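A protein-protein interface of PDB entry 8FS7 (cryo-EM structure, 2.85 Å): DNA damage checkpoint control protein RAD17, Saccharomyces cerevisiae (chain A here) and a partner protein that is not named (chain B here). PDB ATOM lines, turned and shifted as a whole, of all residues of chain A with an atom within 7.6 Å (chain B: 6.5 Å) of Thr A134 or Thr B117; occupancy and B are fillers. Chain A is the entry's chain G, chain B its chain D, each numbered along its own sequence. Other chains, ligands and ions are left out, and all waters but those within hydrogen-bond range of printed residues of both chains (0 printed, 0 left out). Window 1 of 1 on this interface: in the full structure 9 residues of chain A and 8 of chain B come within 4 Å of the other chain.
Among the printed residues, pairs that only touch across the chains: Gly A114 with Val B118 (3.3 Å), Tyr A135 with Arg B115 (3.3 Å), Tyr A135 with Asn B112 (3.4 Å), Tyr A135 with Thr B117 (3.5 Å), Gly A114 with Thr B117 (3.6 Å), Tyr A135 with Leu B116 (3.6 Å), His A113 with Lys B120 (3.6 Å), Gly A114 with Lys B120 (3.6 Å), Leu A136 with Val B163 (3.7 Å), Thr A134 with Leu B116 (3.7 Å), His A113 with Thr B117 (3.7 Å), Ser A133 with Leu B116 (3.7 Å), Leu A136 with Thr B117 (3.95 Å) and Gly A114 with Ser B119 (3.98 Å).
Printed residues of chain B that touch a printed residue of chain A: Asn B112, Arg B115, Leu B116, Thr B117, Val B118, Ser B119, Lys B120 and Val B163.
Along chain B the printed residues that touch a printed residue of chain A span positions 112 to 163.
Printed residues of chain A that touch a printed residue of chain B: Cys A83, His A113, Gly A114, Ser A115, Ser A133, Thr A134, Tyr A135 and Leu A136.
Among the printed residues, 18 pairs touch across the chains.
Among the printed residues, no Asp or Glu carboxylate lies within 4 Å of a Lys or Arg side-chain nitrogen of the other chain.
Of chain A, only His A113, Gly A114, Thr A134, Tyr A135 and Leu A136 come within 4 Å of Thr B117.
Printed residues of chain A within 4 Å of Ser B119: Gly A114.
Of the printed residues of chain B, Leu A136 touches Arg B115, Thr B117 and Val B163.
Of the printed residues of chain A, Asn B112 touches Tyr A135.
Lys A85 touches none of the printed residues of chain B.
Tyr A110 touches none of the printed residues of chain B.
The nearest residue of chain B that does not touch Thr A134 is Arg B115 (4.7 Å).
The nearest printed residue of chain B that does not touch Tyr A135 is Phe B113 (5.4 Å).
The side-chain sulfur (SG) of Cys A83 sits at hydrogen-bond distance from the guanidinium group (NH2) of Arg B115.
The backbone NH (N) of Leu A136 is in hydrogen-bond range of the backbone carbonyl oxygen (O) of Arg B115, 2.7 Å away.
The backbone NH (N) of Thr B117 lies within hydrogen-bond range of the backbone carbonyl oxygen (O) of Thr A134, at 3.0 Å.
The side-chain hydroxyl (OG) of Ser A115 lies close to the side-chain amino group (NZ) of Lys B120 (3.3 Å).
The side-chain amino group of Lys B135 lies within hydrogen-bond range of the backbone carbonyl oxygen of Leu B116 (2.8 Å).
The backbone carbonyl oxygen (O) of Val B163 sits at hydrogen-bond distance from the side-chain amino group (NZ) of Lys B135, 2.7 Å away.
The backbone carbonyl oxygen of Cys A83 sits at hydrogen-bond distance from the backbone NH of Tyr A135, 2.7 Å away.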
ATOM      1  N   LYS A  81     -18.919 -25.338 -11.065  1.00  0.00           N
ATOM      2  CA  LYS A  81     -18.667 -24.429  -9.956  1.00  0.00           C
ATOM      3  C   LYS A  81     -18.999 -23.002 -10.371  1.00  0.00           C
ATOM      4  O   LYS A  81     -18.544 -22.534 -11.421  1.00  0.00           O
ATOM      5  CB  LYS A  81     -17.210 -24.520  -9.499  1.00  0.00           C
ATOM      6  CG  LYS A  81     -16.676 -25.938  -9.382  1.00  0.00           C
ATOM      7  CD  LYS A  81     -15.195 -25.946  -9.027  1.00  0.00           C
ATOM      8  CE  LYS A  81     -14.871 -24.928  -7.943  1.00  0.00           C
ATOM      9  NZ  LYS A  81     -13.997 -25.498  -6.880  1.00  0.00           N
ATOM     10  N   LEU A  82     -19.790 -22.317  -9.548  1.00  0.00           N
ATOM     11  CA  LEU A  82     -20.141 -20.924  -9.782  1.00  0.00           C
ATOM     12  C   LEU A  82     -20.083 -20.165  -8.465  1.00  0.00           C
ATOM     13  O   LEU A  82     -20.429 -20.705  -7.410  1.00  0.00           O
ATOM     14  CB  LEU A  82     -21.533 -20.792 -10.420  1.00  0.00           C
ATOM     15  CG  LEU A  82     -22.756 -21.198  -9.593  1.00  0.00           C
ATOM     16  CD1 LEU A  82     -23.537 -19.972  -9.146  1.00  0.00           C
ATOM     17  CD2 LEU A  82     -23.645 -22.144 -10.384  1.00  0.00           C
ATOM     18  N   CYS A  83     -19.632 -18.915  -8.528  1.00  0.00           N
ATOM     19  CA  CYS A  83     -19.480 -18.063  -7.356  1.00  0.00           C
ATOM     20  C   CYS A  83     -20.381 -16.844  -7.504  1.00  0.00           C
ATOM     21  O   CYS A  83     -20.249 -16.085  -8.469  1.00  0.00           O
ATOM     22  CB  CYS A  83     -18.022 -17.640  -7.177  1.00  0.00           C
ATOM     23  SG  CYS A  83     -17.782 -16.215  -6.097  1.00  0.00           S
ATOM     24  N   VAL A  84     -21.290 -16.657  -6.546  1.00  0.00           N
ATOM     25  CA  VAL A  84     -22.235 -15.548  -6.547  1.00  0.00           C
ATOM     26  C   VAL A  84     -22.351 -15.004  -5.128  1.00  0.00           C
ATOM     27  O   VAL A  84     -21.723 -15.503  -4.192  1.00  0.00           O
ATOM     28  CB  VAL A  84     -23.626 -15.961  -7.076  1.00  0.00           C
ATOM     29  CG1 VAL A  84     -23.586 -16.180  -8.580  1.00  0.00           C
ATOM     30  CG2 VAL A  84     -24.104 -17.215  -6.370  1.00  0.00           C
ATOM     31  N   LYS A  85     -23.159 -13.956  -4.980  1.00  0.00           N
ATOM     32  CA  LYS A  85     -23.434 -13.403  -3.663  1.00  0.00           C
ATOM     33  C   LYS A  85     -24.489 -14.242  -2.944  1.00  0.00           C
ATOM     34  O   LYS A  85     -25.237 -15.009  -3.558  1.00  0.00           O
ATOM     35  CB  LYS A  85     -23.890 -11.949  -3.776  1.00  0.00           C
ATOM     36  CG  LYS A  85     -22.943 -11.069  -4.576  1.00  0.00           C
ATOM     37  CD  LYS A  85     -21.571 -11.000  -3.922  1.00  0.00           C
ATOM     38  CE  LYS A  85     -20.610 -10.147  -4.735  1.00  0.00           C
ATOM     39  NZ  LYS A  85     -19.223 -10.209  -4.198  1.00  0.00           N
ATOM     40  N   TYR A 110     -29.067 -22.894 -14.645  1.00  0.00           N
ATOM     41  CA  TYR A 110     -27.711 -22.454 -14.945  1.00  0.00           C
ATOM     42  C   TYR A 110     -27.313 -23.049 -16.286  1.00  0.00           C
ATOM     43  O   TYR A 110     -27.482 -24.253 -16.501  1.00  0.00           O
ATOM     44  CB  TYR A 110     -26.728 -22.879 -13.849  1.00  0.00           C
ATOM     45  CG  TYR A 110     -25.378 -22.204 -13.940  1.00  0.00           C
ATOM     46  CD1 TYR A 110     -25.262 -20.824 -13.849  1.00  0.00           C
ATOM     47  CD2 TYR A 110     -24.218 -22.946 -14.121  1.00  0.00           C
ATOM     48  CE1 TYR A 110     -24.031 -20.203 -13.932  1.00  0.00           C
ATOM     49  CE2 TYR A 110     -22.983 -22.335 -14.206  1.00  0.00           C
ATOM     50  CZ  TYR A 110     -22.895 -20.962 -14.110  1.00  0.00           C
ATOM     51  OH  TYR A 110     -21.667 -20.348 -14.194  1.00  0.00           O
ATOM     52  N   GLY A 112     -24.180 -23.034 -17.860  1.00  0.00           N
ATOM     53  CA  GLY A 112     -22.748 -23.092 -18.041  1.00  0.00           C
ATOM     54  C   GLY A 112     -22.060 -21.765 -17.778  1.00  0.00           C
ATOM     55  O   GLY A 112     -22.625 -20.821 -17.217  1.00  0.00           O
ATOM     56  N   HIS A 113     -20.797 -21.709 -18.198  1.00  0.00           N
ATOM     57  CA  HIS A 113     -19.985 -20.518 -17.991  1.00  0.00           C
ATOM     58  C   HIS A 113     -20.532 -19.345 -18.796  1.00  0.00           C
ATOM     59  O   HIS A 113     -20.921 -19.493 -19.958  1.00  0.00           O
ATOM     60  CB  HIS A 113     -18.533 -20.796 -18.385  1.00  0.00           C
ATOM     61  CG  HIS A 113     -17.528 -20.080 -17.538  1.00  0.00           C
ATOM     62  ND1 HIS A 113     -16.867 -18.948 -17.965  1.00  0.00           N
ATOM     63  CD2 HIS A 113     -17.068 -20.336 -16.291  1.00  0.00           C
ATOM     64  CE1 HIS A 113     -16.045 -18.537 -17.016  1.00  0.00           C
ATOM     65  NE2 HIS A 113     -16.148 -19.362 -15.990  1.00  0.00           N
ATOM     66  N   GLY A 114     -20.561 -18.171 -18.167  1.00  0.00           N
ATOM     67  CA  GLY A 114     -21.057 -16.969 -18.798  1.00  0.00           C
ATOM     68  C   GLY A 114     -22.543 -16.727 -18.647  1.00  0.00           C
ATOM     69  O   GLY A 114     -23.027 -15.672 -19.076  1.00  0.00           O
ATOM     70  N   SER A 115     -23.281 -17.664 -18.054  1.00  0.00           N
ATOM     71  CA  SER A 115     -24.714 -17.510 -17.879  1.00  0.00           C
ATOM     72  C   SER A 115     -25.043 -17.124 -16.443  1.00  0.00           C
ATOM     73  O   SER A 115     -24.334 -17.511 -15.509  1.00  0.00           O
ATOM     74  CB  SER A 115     -25.442 -18.811 -18.234  1.00  0.00           C
ATOM     75  OG  SER A 115     -25.184 -19.188 -19.574  1.00  0.00           O
ATOM     76  N   PRO A 116     -26.104 -16.351 -16.232  1.00  0.00           N
ATOM     77  CA  PRO A 116     -26.516 -16.017 -14.866  1.00  0.00           C
ATOM     78  C   PRO A 116     -27.225 -17.181 -14.190  1.00  0.00           C
ATOM     79  O   PRO A 116     -27.774 -18.077 -14.832  1.00  0.00           O
ATOM     80  CB  PRO A 116     -27.467 -14.833 -15.064  1.00  0.00           C
ATOM     81  CG  PRO A 116     -28.038 -15.047 -16.420  1.00  0.00           C
ATOM     82  CD  PRO A 116     -26.957 -15.700 -17.242  1.00  0.00           C
ATOM     83  N   PHE A 117     -27.203 -17.148 -12.859  1.00  0.00           N
ATOM     84  CA  PHE A 117     -27.894 -18.146 -12.042  1.00  0.00           C
ATOM     85  C   PHE A 117     -29.331 -17.672 -11.855  1.00  0.00           C
ATOM     86  O   PHE A 117     -29.604 -16.774 -11.055  1.00  0.00           O
ATOM     87  CB  PHE A 117     -27.183 -18.340 -10.708  1.00  0.00           C
ATOM     88  CG  PHE A 117     -27.605 -19.578  -9.970  1.00  0.00           C
ATOM     89  CD1 PHE A 117     -27.481 -20.827 -10.557  1.00  0.00           C
ATOM     90  CD2 PHE A 117     -28.121 -19.496  -8.688  1.00  0.00           C
ATOM     91  CE1 PHE A 117     -27.868 -21.969  -9.880  1.00  0.00           C
ATOM     92  CE2 PHE A 117     -28.509 -20.633  -8.006  1.00  0.00           C
ATOM     93  CZ  PHE A 117     -28.382 -21.871  -8.603  1.00  0.00           C
ATOM     94  N   GLU A 131     -32.097 -13.124 -11.643  1.00  0.00           N
ATOM     95  CA  GLU A 131     -30.856 -13.552 -12.271  1.00  0.00           C
ATOM     96  C   GLU A 131     -29.673 -13.015 -11.480  1.00  0.00           C
ATOM     97  O   GLU A 131     -29.668 -11.851 -11.068  1.00  0.00           O
ATOM     98  CB  GLU A 131     -30.778 -13.071 -13.724  1.00  0.00           C
ATOM     99  CG  GLU A 131     -31.916 -13.564 -14.602  1.00  0.00           C
ATOM    100  CD  GLU A 131     -31.782 -13.105 -16.040  1.00  0.00           C
ATOM    101  OE1 GLU A 131     -30.877 -12.293 -16.325  1.00  0.00           O
ATOM    102  OE2 GLU A 131     -32.584 -13.555 -16.886  1.00  0.00           O
ATOM    103  N   TYR A 132     -28.672 -13.866 -11.267  1.00  0.00           N
ATOM    104  CA  TYR A 132     -27.474 -13.502 -10.525  1.00  0.00           C
ATOM    105  C   TYR A 132     -26.244 -13.773 -11.376  1.00  0.00           C
ATOM    106  O   TYR A 132     -26.041 -14.901 -11.838  1.00  0.00           O
ATOM    107  CB  TYR A 132     -27.381 -14.279  -9.209  1.00  0.00           C
ATOM    108  CG  TYR A 132     -28.519 -14.003  -8.258  1.00  0.00           C
ATOM    109  CD1 TYR A 132     -28.848 -12.703  -7.902  1.00  0.00           C
ATOM    110  CD2 TYR A 132     -29.260 -15.041  -7.710  1.00  0.00           C
ATOM    111  CE1 TYR A 132     -29.888 -12.444  -7.035  1.00  0.00           C
ATOM    112  CE2 TYR A 132     -30.301 -14.792  -6.838  1.00  0.00           C
ATOM    113  CZ  TYR A 132     -30.609 -13.491  -6.503  1.00  0.00           C
ATOM    114  OH  TYR A 132     -31.644 -13.232  -5.635  1.00  0.00           O
ATOM    115  N   SER A 133     -25.426 -12.744 -11.575  1.00  0.00           N
ATOM    116  CA  SER A 133     -24.191 -12.895 -12.329  1.00  0.00           C
ATOM    117  C   SER A 133     -23.140 -13.607 -11.488  1.00  0.00           C
ATOM    118  O   SER A 133     -22.992 -13.339 -10.292  1.00  0.00           O
ATOM    119  CB  SER A 133     -23.668 -11.531 -12.779  1.00  0.00           C
ATOM    120  OG  SER A 133     -24.592 -10.889 -13.640  1.00  0.00           O
ATOM    121  N   THR A 134     -22.409 -14.516 -12.122  1.00  0.00           N
ATOM    122  CA  THR A 134     -21.370 -15.288 -11.458  1.00  0.00           C
ATOM    123  C   THR A 134     -20.029 -14.575 -11.566  1.00  0.00           C
ATOM    124  O   THR A 134     -19.782 -13.814 -12.505  1.00  0.00           O
ATOM    125  CB  THR A 134     -21.264 -16.693 -12.055  1.00  0.00           C
ATOM    126  OG1 THR A 134     -20.731 -16.612 -13.383  1.00  0.00           O
ATOM    127  CG2 THR A 134     -22.633 -17.355 -12.102  1.00  0.00           C
ATOM    128  N   TYR A 135     -19.167 -14.823 -10.586  1.00  0.00           N
ATOM    129  CA  TYR A 135     -17.855 -14.201 -10.510  1.00  0.00           C
ATOM    130  C   TYR A 135     -16.763 -15.230 -10.778  1.00  0.00           C
ATOM    131  O   TYR A 135     -17.005 -16.440 -10.814  1.00  0.00           O
ATOM    132  CB  TYR A 135     -17.644 -13.544  -9.141  1.00  0.00           C
ATOM    133  CG  TYR A 135     -18.510 -12.328  -8.906  1.00  0.00           C
ATOM    134  CD1 TYR A 135     -19.812 -12.457  -8.440  1.00  0.00           C
ATOM    135  CD2 TYR A 135     -18.025 -11.052  -9.151  1.00  0.00           C
ATOM    136  CE1 TYR A 135     -20.606 -11.347  -8.225  1.00  0.00           C
ATOM    137  CE2 TYR A 135     -18.810  -9.935  -8.938  1.00  0.00           C
ATOM    138  CZ  TYR A 135     -20.098 -10.089  -8.476  1.00  0.00           C
ATOM    139  OH  TYR A 135     -20.883  -8.979  -8.262  1.00  0.00           O
ATOM    140  N   LEU A 136     -15.548 -14.727 -10.969  1.00  0.00           N
ATOM    141  CA  LEU A 136     -14.404 -15.597 -11.203  1.00  0.00           C
ATOM    142  C   LEU A 136     -14.069 -16.387  -9.944  1.00  0.00           C
ATOM    143  O   LEU A 136     -14.290 -15.924  -8.821  1.00  0.00           O
ATOM    144  CB  LEU A 136     -13.194 -14.781 -11.654  1.00  0.00           C
ATOM    145  CG  LEU A 136     -12.324 -15.452 -12.718  1.00  0.00           C
ATOM    146  CD1 LEU A 136     -13.088 -15.575 -14.024  1.00  0.00           C
ATOM    147  CD2 LEU A 136     -11.024 -14.687 -12.925  1.00  0.00           C
ATOM    148  N   ILE A 137     -13.535 -17.587 -10.139  1.00  0.00           N
ATOM    149  CA  ILE A 137     -13.264 -18.497  -9.035  1.00  0.00           C
ATOM    150  C   ILE A 137     -11.762 -18.670  -8.822  1.00  0.00           C
ATOM    151  O   ILE A 137     -10.969 -17.787  -9.147  1.00  0.00           O
ATOM    152  CB  ILE A 137     -13.943 -19.854  -9.277  1.00  0.00           C
ATOM    153  CG1 ILE A 137     -15.420 -19.783  -8.883  1.00  0.00           C
ATOM    154  CG2 ILE A 137     -13.226 -20.960  -8.514  1.00  0.00           C
ATOM    155  CD1 ILE A 137     -16.139 -21.103  -8.985  1.00  0.00           C
ATOM    156  N   ASN B 112     -15.696  -5.325  -8.602  1.00  0.00           N
ATOM    157  CA  ASN B 112     -16.790  -6.244  -8.893  1.00  0.00           C
ATOM    158  C   ASN B 112     -16.929  -6.483 -10.391  1.00  0.00           C
ATOM    159  O   ASN B 112     -17.176  -7.616 -10.819  1.00  0.00           O
ATOM    160  CB  ASN B 112     -18.096  -5.707  -8.310  1.00  0.00           C
ATOM    161  CG  ASN B 112     -18.184  -5.896  -6.809  1.00  0.00           C
ATOM    162  OD1 ASN B 112     -17.274  -6.443  -6.186  1.00  0.00           O
ATOM    163  ND2 ASN B 112     -19.283  -5.441  -6.218  1.00  0.00           N
ATOM    164  N   PHE B 113     -16.786  -5.431 -11.203  1.00  0.00           N
ATOM    165  CA  PHE B 113     -16.875  -5.614 -12.649  1.00  0.00           C
ATOM    166  C   PHE B 113     -15.723  -6.462 -13.171  1.00  0.00           C
ATOM    167  O   PHE B 113     -15.921  -7.312 -14.046  1.00  0.00           O
ATOM    168  CB  PHE B 113     -16.910  -4.263 -13.361  1.00  0.00           C
ATOM    169  CG  PHE B 113     -17.331  -4.355 -14.800  1.00  0.00           C
ATOM    170  CD1 PHE B 113     -18.674  -4.400 -15.140  1.00  0.00           C
ATOM    171  CD2 PHE B 113     -16.388  -4.416 -15.812  1.00  0.00           C
ATOM    172  CE1 PHE B 113     -19.066  -4.492 -16.461  1.00  0.00           C
ATOM    173  CE2 PHE B 113     -16.775  -4.510 -17.136  1.00  0.00           C
ATOM    174  CZ  PHE B 113     -18.116  -4.547 -17.461  1.00  0.00           C
ATOM    175  N   ALA B 114     -14.511  -6.246 -12.651  1.00  0.00           N
ATOM    176  CA  ALA B 114     -13.376  -7.062 -13.067  1.00  0.00           C
ATOM    177  C   ALA B 114     -13.525  -8.505 -12.606  1.00  0.00           C
ATOM    178  O   ALA B 114     -13.085  -9.428 -13.301  1.00  0.00           O
ATOM    179  CB  ALA B 114     -12.074  -6.464 -12.532  1.00  0.00           C
ATOM    180  N   ARG B 115     -14.140  -8.721 -11.442  1.00  0.00           N
ATOM    181  CA  ARG B 115     -14.337 -10.072 -10.931  1.00  0.00           C
ATOM    182  C   ARG B 115     -15.449 -10.812 -11.663  1.00  0.00           C
ATOM    183  O   ARG B 115     -15.571 -12.033 -11.519  1.00  0.00           O
ATOM    184  CB  ARG B 115     -14.642 -10.023  -9.433  1.00  0.00           C
ATOM    185  CG  ARG B 115     -13.497 -10.472  -8.544  1.00  0.00           C
ATOM    186  CD  ARG B 115     -13.952 -10.658  -7.102  1.00  0.00           C
ATOM    187  NE  ARG B 115     -14.747 -11.867  -6.920  1.00  0.00           N
ATOM    188  CZ  ARG B 115     -14.245 -13.092  -6.833  1.00  0.00           C
ATOM    189  NH1 ARG B 115     -12.943 -13.312  -6.896  1.00  0.00           N
ATOM    190  NH2 ARG B 115     -15.072 -14.121  -6.674  1.00  0.00           N
ATOM    191  N   LEU B 116     -16.264 -10.099 -12.438  1.00  0.00           N
ATOM    192  CA  LEU B 116     -17.403 -10.714 -13.108  1.00  0.00           C
ATOM    193  C   LEU B 116     -16.946 -11.691 -14.186  1.00  0.00           C
ATOM    194  O   LEU B 116     -15.896 -11.522 -14.810  1.00  0.00           O
ATOM    195  CB  LEU B 116     -18.301  -9.640 -13.722  1.00  0.00           C
ATOM    196  CG  LEU B 116     -19.367  -9.051 -12.799  1.00  0.00           C
ATOM    197  CD1 LEU B 116     -20.203  -8.015 -13.533  1.00  0.00           C
ATOM    198  CD2 LEU B 116     -20.244 -10.160 -12.247  1.00  0.00           C
ATOM    199  N   THR B 117     -17.750 -12.733 -14.389  1.00  0.00           N
ATOM    200  CA  THR B 117     -17.488 -13.702 -15.444  1.00  0.00           C
ATOM    201  C   THR B 117     -17.860 -13.103 -16.800  1.00  0.00           C
ATOM    202  O   THR B 117     -18.826 -12.345 -16.926  1.00  0.00           O
ATOM    203  CB  THR B 117     -18.267 -14.999 -15.161  1.00  0.00           C
ATOM    204  OG1 THR B 117     -17.541 -15.792 -14.214  1.00  0.00           O
ATOM    205  CG2 THR B 117     -18.503 -15.836 -16.420  1.00  0.00           C
ATOM    206  N   VAL B 118     -17.071 -13.445 -17.817  1.00  0.00           N
ATOM    207  CA  VAL B 118     -17.276 -12.927 -19.165  1.00  0.00           C
ATOM    208  C   VAL B 118     -18.593 -13.457 -19.715  1.00  0.00           C
ATOM    209  O   VAL B 118     -18.868 -14.661 -19.650  1.00  0.00           O
ATOM    210  CB  VAL B 118     -16.104 -13.318 -20.076  1.00  0.00           C
ATOM    211  CG1 VAL B 118     -16.133 -12.510 -21.355  1.00  0.00           C
ATOM    212  CG2 VAL B 118     -14.793 -13.118 -19.352  1.00  0.00           C
ATOM    213  N   SER B 119     -19.410 -12.556 -20.259  1.00  0.00           N
ATOM    214  CA  SER B 119     -20.705 -12.939 -20.803  1.00  0.00           C
ATOM    215  C   SER B 119     -20.535 -13.805 -22.047  1.00  0.00           C
ATOM    216  O   SER B 119     -19.600 -13.631 -22.832  1.00  0.00           O
ATOM    217  CB  SER B 119     -21.527 -11.694 -21.138  1.00  0.00           C
ATOM    218  OG  SER B 119     -22.349 -11.315 -20.048  1.00  0.00           O
ATOM    219  N   LYS B 120     -21.455 -14.747 -22.220  1.00  0.00           N
ATOM    220  CA  LYS B 120     -21.387 -15.669 -23.346  1.00  0.00           C
ATOM    221  C   LYS B 120     -21.843 -14.970 -24.621  1.00  0.00           C
ATOM    222  O   LYS B 120     -22.966 -14.455 -24.664  1.00  0.00           O
ATOM    223  CB  LYS B 120     -22.252 -16.896 -23.085  1.00  0.00           C
ATOM    224  CG  LYS B 120     -21.599 -18.211 -23.484  1.00  0.00           C
ATOM    225  CD  LYS B 120     -22.620 -19.335 -23.596  1.00  0.00           C
ATOM    226  CE  LYS B 120     -23.585 -19.334 -22.423  1.00  0.00           C
ATOM    227  NZ  LYS B 120     -24.697 -20.308 -22.610  1.00  0.00           N
ATOM    228  N   LYS B 135     -13.039  -8.600 -21.121  1.00  0.00           N
ATOM    229  CA  LYS B 135     -13.816  -7.372 -21.193  1.00  0.00           C
ATOM    230  C   LYS B 135     -12.907  -6.189 -20.891  1.00  0.00           C
ATOM    231  O   LYS B 135     -11.823  -6.342 -20.323  1.00  0.00           O
ATOM    232  CB  LYS B 135     -15.007  -7.396 -20.224  1.00  0.00           C
ATOM    233  CG  LYS B 135     -14.658  -7.830 -18.816  1.00  0.00           C
ATOM    234  CD  LYS B 135     -15.899  -8.289 -18.073  1.00  0.00           C
ATOM    235  CE  LYS B 135     -15.535  -8.962 -16.766  1.00  0.00           C
ATOM    236  NZ  LYS B 135     -14.703 -10.177 -16.982  1.00  0.00           N
ATOM    237  N   VAL B 163      -9.107 -11.785 -17.399  1.00  0.00           N
ATOM    238  CA  VAL B 163     -10.561 -11.791 -17.501  1.00  0.00           C
ATOM    239  C   VAL B 163     -11.053 -10.372 -17.752  1.00  0.00           C
ATOM    240  O   VAL B 163     -12.211 -10.161 -18.134  1.00  0.00           O
ATOM    241  CB  VAL B 163     -11.195 -12.394 -16.232  1.00  0.00           C
ATOM    242  CG1 VAL B 163     -11.210 -11.379 -15.103  1.00  0.00           C
ATOM    243  CG2 VAL B 163     -12.595 -12.907 -16.518  1.00  0.00           C
